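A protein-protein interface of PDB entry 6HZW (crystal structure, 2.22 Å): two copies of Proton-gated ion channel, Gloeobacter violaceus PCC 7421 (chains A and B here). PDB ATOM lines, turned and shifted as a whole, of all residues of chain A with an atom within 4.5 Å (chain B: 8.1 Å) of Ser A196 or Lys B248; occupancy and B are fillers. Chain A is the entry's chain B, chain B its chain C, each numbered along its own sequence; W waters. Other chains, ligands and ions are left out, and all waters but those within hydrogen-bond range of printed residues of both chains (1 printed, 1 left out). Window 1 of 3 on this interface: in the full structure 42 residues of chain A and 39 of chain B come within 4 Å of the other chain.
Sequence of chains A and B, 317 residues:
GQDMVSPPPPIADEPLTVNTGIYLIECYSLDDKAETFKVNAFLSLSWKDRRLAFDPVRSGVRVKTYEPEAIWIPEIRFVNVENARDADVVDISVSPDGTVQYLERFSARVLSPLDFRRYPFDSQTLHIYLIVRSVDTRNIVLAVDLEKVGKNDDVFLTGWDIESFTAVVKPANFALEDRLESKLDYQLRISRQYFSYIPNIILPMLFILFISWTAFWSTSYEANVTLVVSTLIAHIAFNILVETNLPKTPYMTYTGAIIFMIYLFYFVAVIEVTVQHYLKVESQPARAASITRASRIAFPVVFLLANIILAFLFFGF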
ATOM      1  N   GLY A 159       2.441  30.074 -24.546  1.00  0.00           N
ATOM      2  CA  GLY A 159       3.685  30.046 -25.312  1.00  0.00           C
ATOM      3  C   GLY A 159       4.488  31.344 -25.283  1.00  0.00           C
ATOM      4  O   GLY A 159       5.551  31.409 -25.894  1.00  0.00           O
ATOM      5  N   TYR A 194      10.895  29.979 -25.408  1.00  0.00           N
ATOM      6  CA  TYR A 194      11.692  29.116 -26.293  1.00  0.00           C
ATOM      7  C   TYR A 194      11.926  27.682 -25.719  1.00  0.00           C
ATOM      8  O   TYR A 194      12.342  26.783 -26.467  1.00  0.00           O
ATOM      9  CB  TYR A 194      13.012  29.800 -26.685  1.00  0.00           C
ATOM     10  CG  TYR A 194      13.823  30.148 -25.510  1.00  0.00           C
ATOM     11  CD1 TYR A 194      14.554  29.183 -24.886  1.00  0.00           C
ATOM     12  CD2 TYR A 194      13.833  31.462 -25.000  1.00  0.00           C
ATOM     13  CE1 TYR A 194      15.278  29.470 -23.771  1.00  0.00           C
ATOM     14  CE2 TYR A 194      14.572  31.764 -23.894  1.00  0.00           C
ATOM     15  CZ  TYR A 194      15.275  30.749 -23.292  1.00  0.00           C
ATOM     16  OH  TYR A 194      16.029  30.948 -22.209  1.00  0.00           O
ATOM     17  N   PHE A 195      11.674  27.502 -24.420  1.00  0.00           N
ATOM     18  CA  PHE A 195      11.971  26.260 -23.685  1.00  0.00           C
ATOM     19  C   PHE A 195      11.702  24.966 -24.458  1.00  0.00           C
ATOM     20  O   PHE A 195      12.642  24.207 -24.665  1.00  0.00           O
ATOM     21  CB  PHE A 195      11.226  26.175 -22.350  1.00  0.00           C
ATOM     22  CG  PHE A 195      11.544  24.926 -21.543  1.00  0.00           C
ATOM     23  CD1 PHE A 195      10.814  23.762 -21.701  1.00  0.00           C
ATOM     24  CD2 PHE A 195      12.553  24.936 -20.624  1.00  0.00           C
ATOM     25  CE1 PHE A 195      11.082  22.635 -20.934  1.00  0.00           C
ATOM     26  CE2 PHE A 195      12.829  23.823 -19.850  1.00  0.00           C
ATOM     27  CZ  PHE A 195      12.111  22.657 -20.026  1.00  0.00           C
ATOM     28  N   SER A 196      10.441  24.692 -24.830  1.00  0.00           N
ATOM     29  CA  SER A 196      10.017  23.454 -25.444  1.00  0.00           C
ATOM     30  C   SER A 196      10.681  23.149 -26.803  1.00  0.00           C
ATOM     31  O   SER A 196      10.728  21.957 -27.169  1.00  0.00           O
ATOM     32  CB  SER A 196       8.485  23.468 -25.596  1.00  0.00           C
ATOM     33  OG  SER A 196       8.160  24.544 -26.438  1.00  0.00           O
ATOM     34  N   TYR A 197      11.176  24.183 -27.511  1.00  0.00           N
ATOM     35  CA  TYR A 197      11.853  24.009 -28.787  1.00  0.00           C
ATOM     36  C   TYR A 197      13.170  23.176 -28.646  1.00  0.00           C
ATOM     37  O   TYR A 197      13.584  22.496 -29.589  1.00  0.00           O
ATOM     38  CB  TYR A 197      12.108  25.335 -29.516  1.00  0.00           C
ATOM     39  CG  TYR A 197      10.850  26.007 -29.907  1.00  0.00           C
ATOM     40  CD1 TYR A 197      10.353  25.853 -31.166  1.00  0.00           C
ATOM     41  CD2 TYR A 197      10.128  26.797 -28.999  1.00  0.00           C
ATOM     42  CE1 TYR A 197       9.144  26.441 -31.545  1.00  0.00           C
ATOM     43  CE2 TYR A 197       8.926  27.401 -29.354  1.00  0.00           C
ATOM     44  CZ  TYR A 197       8.439  27.227 -30.633  1.00  0.00           C
ATOM     45  OH  TYR A 197       7.258  27.814 -31.011  1.00  0.00           O
ATOM     46  N   ILE A 198      13.790  23.266 -27.453  1.00  0.00           N
ATOM     47  CA  ILE A 198      15.014  22.570 -27.151  1.00  0.00           C
ATOM     48  C   ILE A 198      14.859  21.039 -27.123  1.00  0.00           C
ATOM     49  O   ILE A 198      15.484  20.385 -27.940  1.00  0.00           O
ATOM     50  CB  ILE A 198      15.681  23.153 -25.921  1.00  0.00           C
ATOM     51  CG1 ILE A 198      16.071  24.615 -26.248  1.00  0.00           C
ATOM     52  CG2 ILE A 198      16.914  22.321 -25.493  1.00  0.00           C
ATOM     53  CD1 ILE A 198      16.386  25.440 -25.013  1.00  0.00           C
ATOM     54  N   PRO A 199      14.027  20.446 -26.231  1.00  0.00           N
ATOM     55  CA  PRO A 199      13.814  18.983 -26.215  1.00  0.00           C
ATOM     56  C   PRO A 199      13.035  18.434 -27.420  1.00  0.00           C
ATOM     57  O   PRO A 199      13.196  17.259 -27.789  1.00  0.00           O
ATOM     58  CB  PRO A 199      13.038  18.742 -24.927  1.00  0.00           C
ATOM     59  CG  PRO A 199      12.410  20.046 -24.638  1.00  0.00           C
ATOM     60  CD  PRO A 199      13.340  21.093 -25.120  1.00  0.00           C
ATOM     61  N   ASN A 200      12.179  19.249 -28.017  1.00  0.00           N
ATOM     62  CA  ASN A 200      11.307  18.807 -29.132  1.00  0.00           C
ATOM     63  C   ASN A 200      11.817  18.946 -30.572  1.00  0.00           C
ATOM     64  O   ASN A 200      11.471  18.145 -31.373  1.00  0.00           O
ATOM     65  CB  ASN A 200       9.974  19.521 -29.060  1.00  0.00           C
ATOM     66  CG  ASN A 200       9.108  18.984 -27.929  1.00  0.00           C
ATOM     67  OD1 ASN A 200       8.824  17.757 -27.852  1.00  0.00           O
ATOM     68  ND2 ASN A 200       8.666  19.861 -27.084  1.00  0.00           N
ATOM     69  N   ASN A 245       4.646  25.620 -38.684  1.00  0.00           N
ATOM     70  CA  ASN A 245       4.407  26.477 -37.536  1.00  0.00           C
ATOM     71  C   ASN A 245       4.662  27.921 -37.897  1.00  0.00           C
ATOM     72  O   ASN A 245       4.364  28.793 -37.145  1.00  0.00           O
ATOM     73  CB  ASN A 245       5.422  26.207 -36.342  1.00  0.00           C
ATOM     74  CG  ASN A 245       5.352  24.797 -35.688  1.00  0.00           C
ATOM     75  OD1 ASN A 245       4.350  24.084 -35.819  1.00  0.00           O
ATOM     76  ND2 ASN A 245       6.460  24.408 -34.944  1.00  0.00           N
ATOM     77  N   ASP B  32      -7.001  20.840 -25.425  1.00  0.00           N
ATOM     78  CA  ASP B  32      -5.719  20.901 -24.701  1.00  0.00           C
ATOM     79  C   ASP B  32      -4.792  21.998 -25.237  1.00  0.00           C
ATOM     80  O   ASP B  32      -4.209  22.756 -24.433  1.00  0.00           O
ATOM     81  CB  ASP B  32      -4.986  19.537 -24.687  1.00  0.00           C
ATOM     82  CG  ASP B  32      -5.691  18.449 -23.807  1.00  0.00           C
ATOM     83  OD1 ASP B  32      -5.700  18.544 -22.590  1.00  0.00           O
ATOM     84  OD2 ASP B  32      -6.248  17.481 -24.337  1.00  0.00           O
ATOM     85  N   LYS B  33      -4.645  22.072 -26.561  1.00  0.00           N
ATOM     86  CA  LYS B  33      -3.799  23.084 -27.221  1.00  0.00           C
ATOM     87  C   LYS B  33      -4.267  24.483 -26.968  1.00  0.00           C
ATOM     88  O   LYS B  33      -3.440  25.332 -26.650  1.00  0.00           O
ATOM     89  CB  LYS B  33      -3.777  22.886 -28.720  1.00  0.00           C
ATOM     90  CG  LYS B  33      -2.569  22.213 -29.266  1.00  0.00           C
ATOM     91  CD  LYS B  33      -2.826  21.772 -30.714  1.00  0.00           C
ATOM     92  CE  LYS B  33      -1.721  22.226 -31.664  1.00  0.00           C
ATOM     93  NZ  LYS B  33      -0.385  21.760 -31.177  1.00  0.00           N
ATOM     94  N   GLU B  35      -6.424  25.369 -24.550  1.00  0.00           N
ATOM     95  CA  GLU B  35      -6.719  25.484 -23.121  1.00  0.00           C
ATOM     96  C   GLU B  35      -8.105  26.074 -22.890  1.00  0.00           C
ATOM     97  O   GLU B  35      -8.319  26.945 -22.025  1.00  0.00           O
ATOM     98  CB  GLU B  35      -5.619  26.230 -22.376  1.00  0.00           C
ATOM     99  CG  GLU B  35      -4.324  25.417 -22.454  1.00  0.00           C
ATOM    100  CD  GLU B  35      -3.172  25.908 -21.617  1.00  0.00           C
ATOM    101  OE1 GLU B  35      -2.067  25.942 -22.155  1.00  0.00           O
ATOM    102  OE2 GLU B  35      -3.324  26.230 -20.429  1.00  0.00           O
ATOM    103  N   PHE B 116       0.142  20.611 -17.577  1.00  0.00           N
ATOM    104  CA  PHE B 116       0.472  19.354 -18.301  1.00  0.00           C
ATOM    105  C   PHE B 116       1.641  18.529 -17.730  1.00  0.00           C
ATOM    106  O   PHE B 116       1.976  17.507 -18.333  1.00  0.00           O
ATOM    107  CB  PHE B 116       0.741  19.640 -19.797  1.00  0.00           C
ATOM    108  CG  PHE B 116      -0.431  20.120 -20.524  1.00  0.00           C
ATOM    109  CD1 PHE B 116      -1.386  19.235 -20.991  1.00  0.00           C
ATOM    110  CD2 PHE B 116      -0.638  21.510 -20.703  1.00  0.00           C
ATOM    111  CE1 PHE B 116      -2.511  19.710 -21.623  1.00  0.00           C
ATOM    112  CE2 PHE B 116      -1.741  21.989 -21.374  1.00  0.00           C
ATOM    113  CZ  PHE B 116      -2.677  21.081 -21.859  1.00  0.00           C
ATOM    114  N   ASN B 239       7.038  11.048 -31.265  1.00  0.00           N
ATOM    115  CA  ASN B 239       7.358  12.321 -30.636  1.00  0.00           C
ATOM    116  C   ASN B 239       6.520  13.453 -31.332  1.00  0.00           C
ATOM    117  O   ASN B 239       5.907  14.264 -30.641  1.00  0.00           O
ATOM    118  CB  ASN B 239       8.858  12.650 -30.789  1.00  0.00           C
ATOM    119  CG  ASN B 239       9.297  13.898 -30.033  1.00  0.00           C
ATOM    120  OD1 ASN B 239       8.481  14.589 -29.408  1.00  0.00           O
ATOM    121  ND2 ASN B 239      10.575  14.231 -30.129  1.00  0.00           N
ATOM    122  N   GLU B 243       3.422  15.755 -29.623  1.00  0.00           N
ATOM    123  CA  GLU B 243       3.518  17.185 -29.535  1.00  0.00           C
ATOM    124  C   GLU B 243       2.409  17.960 -30.340  1.00  0.00           C
ATOM    125  O   GLU B 243       2.132  19.124 -30.049  1.00  0.00           O
ATOM    126  CB  GLU B 243       5.000  17.612 -29.720  1.00  0.00           C
ATOM    127  CG  GLU B 243       5.380  18.029 -31.112  1.00  0.00           C
ATOM    128  CD  GLU B 243       6.907  18.188 -31.338  1.00  0.00           C
ATOM    129  OE1 GLU B 243       7.726  17.426 -30.753  1.00  0.00           O
ATOM    130  OE2 GLU B 243       7.299  19.087 -32.122  1.00  0.00           O
ATOM    131  N   ASN B 245      -0.742  17.083 -30.116  1.00  0.00           N
ATOM    132  CA  ASN B 245      -1.839  16.976 -29.191  1.00  0.00           C
ATOM    133  C   ASN B 245      -1.685  17.942 -28.043  1.00  0.00           C
ATOM    134  O   ASN B 245      -2.588  18.147 -27.283  1.00  0.00           O
ATOM    135  CB  ASN B 245      -1.962  15.567 -28.477  1.00  0.00           C
ATOM    136  CG  ASN B 245      -2.237  14.355 -29.411  1.00  0.00           C
ATOM    137  OD1 ASN B 245      -2.709  14.513 -30.539  1.00  0.00           O
ATOM    138  ND2 ASN B 245      -1.957  13.108 -28.904  1.00  0.00           N
ATOM    139  N   LEU B 246      -0.529  18.536 -27.918  1.00  0.00           N
ATOM    140  CA  LEU B 246      -0.178  19.391 -26.782  1.00  0.00           C
ATOM    141  C   LEU B 246       0.300  20.795 -27.145  1.00  0.00           C
ATOM    142  O   LEU B 246       0.973  20.965 -28.167  1.00  0.00           O
ATOM    143  CB  LEU B 246       0.986  18.839 -26.030  1.00  0.00           C
ATOM    144  CG  LEU B 246       0.737  17.561 -25.235  1.00  0.00           C
ATOM    145  CD1 LEU B 246       2.067  17.028 -24.776  1.00  0.00           C
ATOM    146  CD2 LEU B 246      -0.138  17.806 -24.010  1.00  0.00           C
ATOM    147  N   PRO B 247      -0.024  21.800 -26.294  1.00  0.00           N
ATOM    148  CA  PRO B 247       0.597  23.111 -26.445  1.00  0.00           C
ATOM    149  C   PRO B 247       2.099  23.081 -26.084  1.00  0.00           C
ATOM    150  O   PRO B 247       2.593  22.178 -25.453  1.00  0.00           O
ATOM    151  CB  PRO B 247      -0.162  23.987 -25.434  1.00  0.00           C
ATOM    152  CG  PRO B 247      -0.556  23.027 -24.379  1.00  0.00           C
ATOM    153  CD  PRO B 247      -0.755  21.694 -25.027  1.00  0.00           C
ATOM    154  N   LYS B 248       2.801  24.124 -26.444  1.00  0.00           N
ATOM    155  CA  LYS B 248       4.199  24.274 -26.064  1.00  0.00           C
ATOM    156  C   LYS B 248       4.194  24.752 -24.605  1.00  0.00           C
ATOM    157  O   LYS B 248       3.507  25.763 -24.266  1.00  0.00           O
ATOM    158  CB  LYS B 248       4.827  25.290 -27.001  1.00  0.00           C
ATOM    159  CG  LYS B 248       5.123  24.553 -28.281  1.00  0.00           C
ATOM    160  CD  LYS B 248       5.207  25.397 -29.507  1.00  0.00           C
ATOM    161  CE  LYS B 248       5.639  24.468 -30.614  1.00  0.00           C
ATOM    162  NZ  LYS B 248       5.000  24.886 -31.861  1.00  0.00           N
ATOM    163  N   THR B 249       4.945  24.069 -23.753  1.00  0.00           N
ATOM    164  CA  THR B 249       4.999  24.420 -22.318  1.00  0.00           C
ATOM    165  C   THR B 249       6.369  24.940 -21.862  1.00  0.00           C
ATOM    166  O   THR B 249       7.388  24.445 -22.332  1.00  0.00           O
ATOM    167  CB  THR B 249       4.591  23.220 -21.463  1.00  0.00           C
ATOM    168  OG1 THR B 249       5.383  22.099 -21.819  1.00  0.00           O
ATOM    169  CG2 THR B 249       3.140  22.882 -21.712  1.00  0.00           C
ATOM    170  N   PRO B 250       6.413  25.875 -20.893  1.00  0.00           N
ATOM    171  CA  PRO B 250       7.746  26.339 -20.412  1.00  0.00           C
ATOM    172  C   PRO B 250       8.345  25.388 -19.364  1.00  0.00           C
ATOM    173  O   PRO B 250       9.184  25.765 -18.584  1.00  0.00           O
ATOM    174  CB  PRO B 250       7.435  27.736 -19.845  1.00  0.00           C
ATOM    175  CG  PRO B 250       6.024  27.668 -19.370  1.00  0.00           C
ATOM    176  CD  PRO B 250       5.322  26.616 -20.218  1.00  0.00           C
ATOM    177  N   TYR B 251       7.906  24.134 -19.379  1.00  0.00           N
ATOM    178  CA  TYR B 251       8.346  23.056 -18.489  1.00  0.00           C
ATOM    179  C   TYR B 251       8.260  21.730 -19.202  1.00  0.00           C
ATOM    180  O   TYR B 251       7.581  21.649 -20.260  1.00  0.00           O
ATOM    181  CB  TYR B 251       7.456  22.987 -17.205  1.00  0.00           C
ATOM    182  CG  TYR B 251       5.975  22.964 -17.472  1.00  0.00           C
ATOM    183  CD1 TYR B 251       5.194  24.144 -17.449  1.00  0.00           C
ATOM    184  CD2 TYR B 251       5.346  21.769 -17.788  1.00  0.00           C
ATOM    185  CE1 TYR B 251       3.808  24.113 -17.721  1.00  0.00           C
ATOM    186  CE2 TYR B 251       3.975  21.734 -18.063  1.00  0.00           C
ATOM    187  CZ  TYR B 251       3.204  22.916 -18.023  1.00  0.00           C
ATOM    188  OH  TYR B 251       1.858  22.768 -18.289  1.00  0.00           O
ATOM    189  N   MET B 252       8.897  20.686 -18.636  1.00  0.00           N
ATOM    190  CA  MET B 252       8.832  19.337 -19.196  1.00  0.00           C
ATOM    191  C   MET B 252       7.560  18.630 -18.693  1.00  0.00           C
ATOM    192  O   MET B 252       7.236  18.731 -17.512  1.00  0.00           O
ATOM    193  CB  MET B 252      10.024  18.459 -18.787  1.00  0.00           C
ATOM    194  CG  MET B 252      11.370  18.870 -19.381  1.00  0.00           C
ATOM    195  SD  MET B 252      11.412  18.792 -21.184  1.00  0.00           S
ATOM    196  CE  MET B 252      11.389  17.030 -21.463  1.00  0.00           C
ATOM    197  N   THR B 253       6.843  17.945 -19.571  1.00  0.00           N
ATOM    198  CA  THR B 253       5.771  17.066 -19.183  1.00  0.00           C
ATOM    199  C   THR B 253       6.373  15.668 -18.936  1.00  0.00           C
ATOM    200  O   THR B 253       7.494  15.386 -19.389  1.00  0.00           O
ATOM    201  CB  THR B 253       4.700  16.945 -20.244  1.00  0.00           C
ATOM    202  OG1 THR B 253       5.251  16.317 -21.385  1.00  0.00           O
ATOM    203  CG2 THR B 253       4.162  18.284 -20.603  1.00  0.00           C
HETATM  204  O   HOH W   1      11.543  15.136 -27.548  1.00  0.00           O
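OD1 of Asn A200 lies close to OE1 of Glu B243 (3.1 Å). The side-chain amide nitrogen (ND2) of Asn A245 lies close to the side-chain amino group (NZ) of Lys B248, at 3.4 Å.
O of Ser A196 sits at hydrogen-bond distance from ND2 of Asn A200 (2.9 Å). The backbone NH (N) of Phe B116 is in hydrogen-bond range of the side-chain hydroxyl (OH) of Tyr B251, at 2.8 Å. The side-chain amide oxygen (OD1) of Asn B239 lies close to the side-chain carboxylate (OE1) of Glu B243, 3.2 Å away. The side-chain hydroxyl (OG1) of Thr B249 lies within hydrogen-bond range of the backbone carbonyl oxygen (O) of Tyr B251 (2.7 Å).
Among the printed residues, pairs that only touch across the chains: Phe A195 with Thr B249 (3.5 Å), Phe A195 with Pro B250 (3.8 Å), Phe A195 with Tyr B251 (3.4 Å), Phe A195 with Met B252 (3.7 Å), Ser A196 with Lys B248 (3.5 Å), Ser A196 with Thr B249 (3.6 Å), Tyr A197 with Lys B248 (3.5 Å), Pro A199 with Met B252 (3.8 Å) and Asn A200 with Asn B239 (3.5 Å).
Of chain B, only Lys B248 and Thr B249 come within 4 Å of Ser A196. Of chain A, only Ser A196 (3.5 Å), Tyr A197 (3.5 Å) and Asn A245 (3.4 Å) come within 4 Å of Lys B248. Of the printed residues of chain B, Asn A200 touches Asn B239 and Glu B243. Printed residues of chain A within 4 Å of Glu B243: Asn A200. Of the printed residues of chain B, Pro A199 touches Met B252 (3.8 Å). The nearest printed residue of chain B that does not touch Tyr A197 is Thr B249 (6.4 Å).
Hydrophobic or aromatic side chains of chain A that line the printed part of chain B: Phe A195, Tyr A197 and Pro A199. Hydrophobic or aromatic side chains of chain B that line the printed part of chain A: Met B252.
Position printed for both chains: 245. Of the 11 pairs that touch across the chains among the printed residues, none has its exchanged pair printed and touching as well.
Water W1 lies within hydrogen-bond range of O of Pro A199 (2.7 Å) and ND2 of Asn B239 (2.9 Å).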
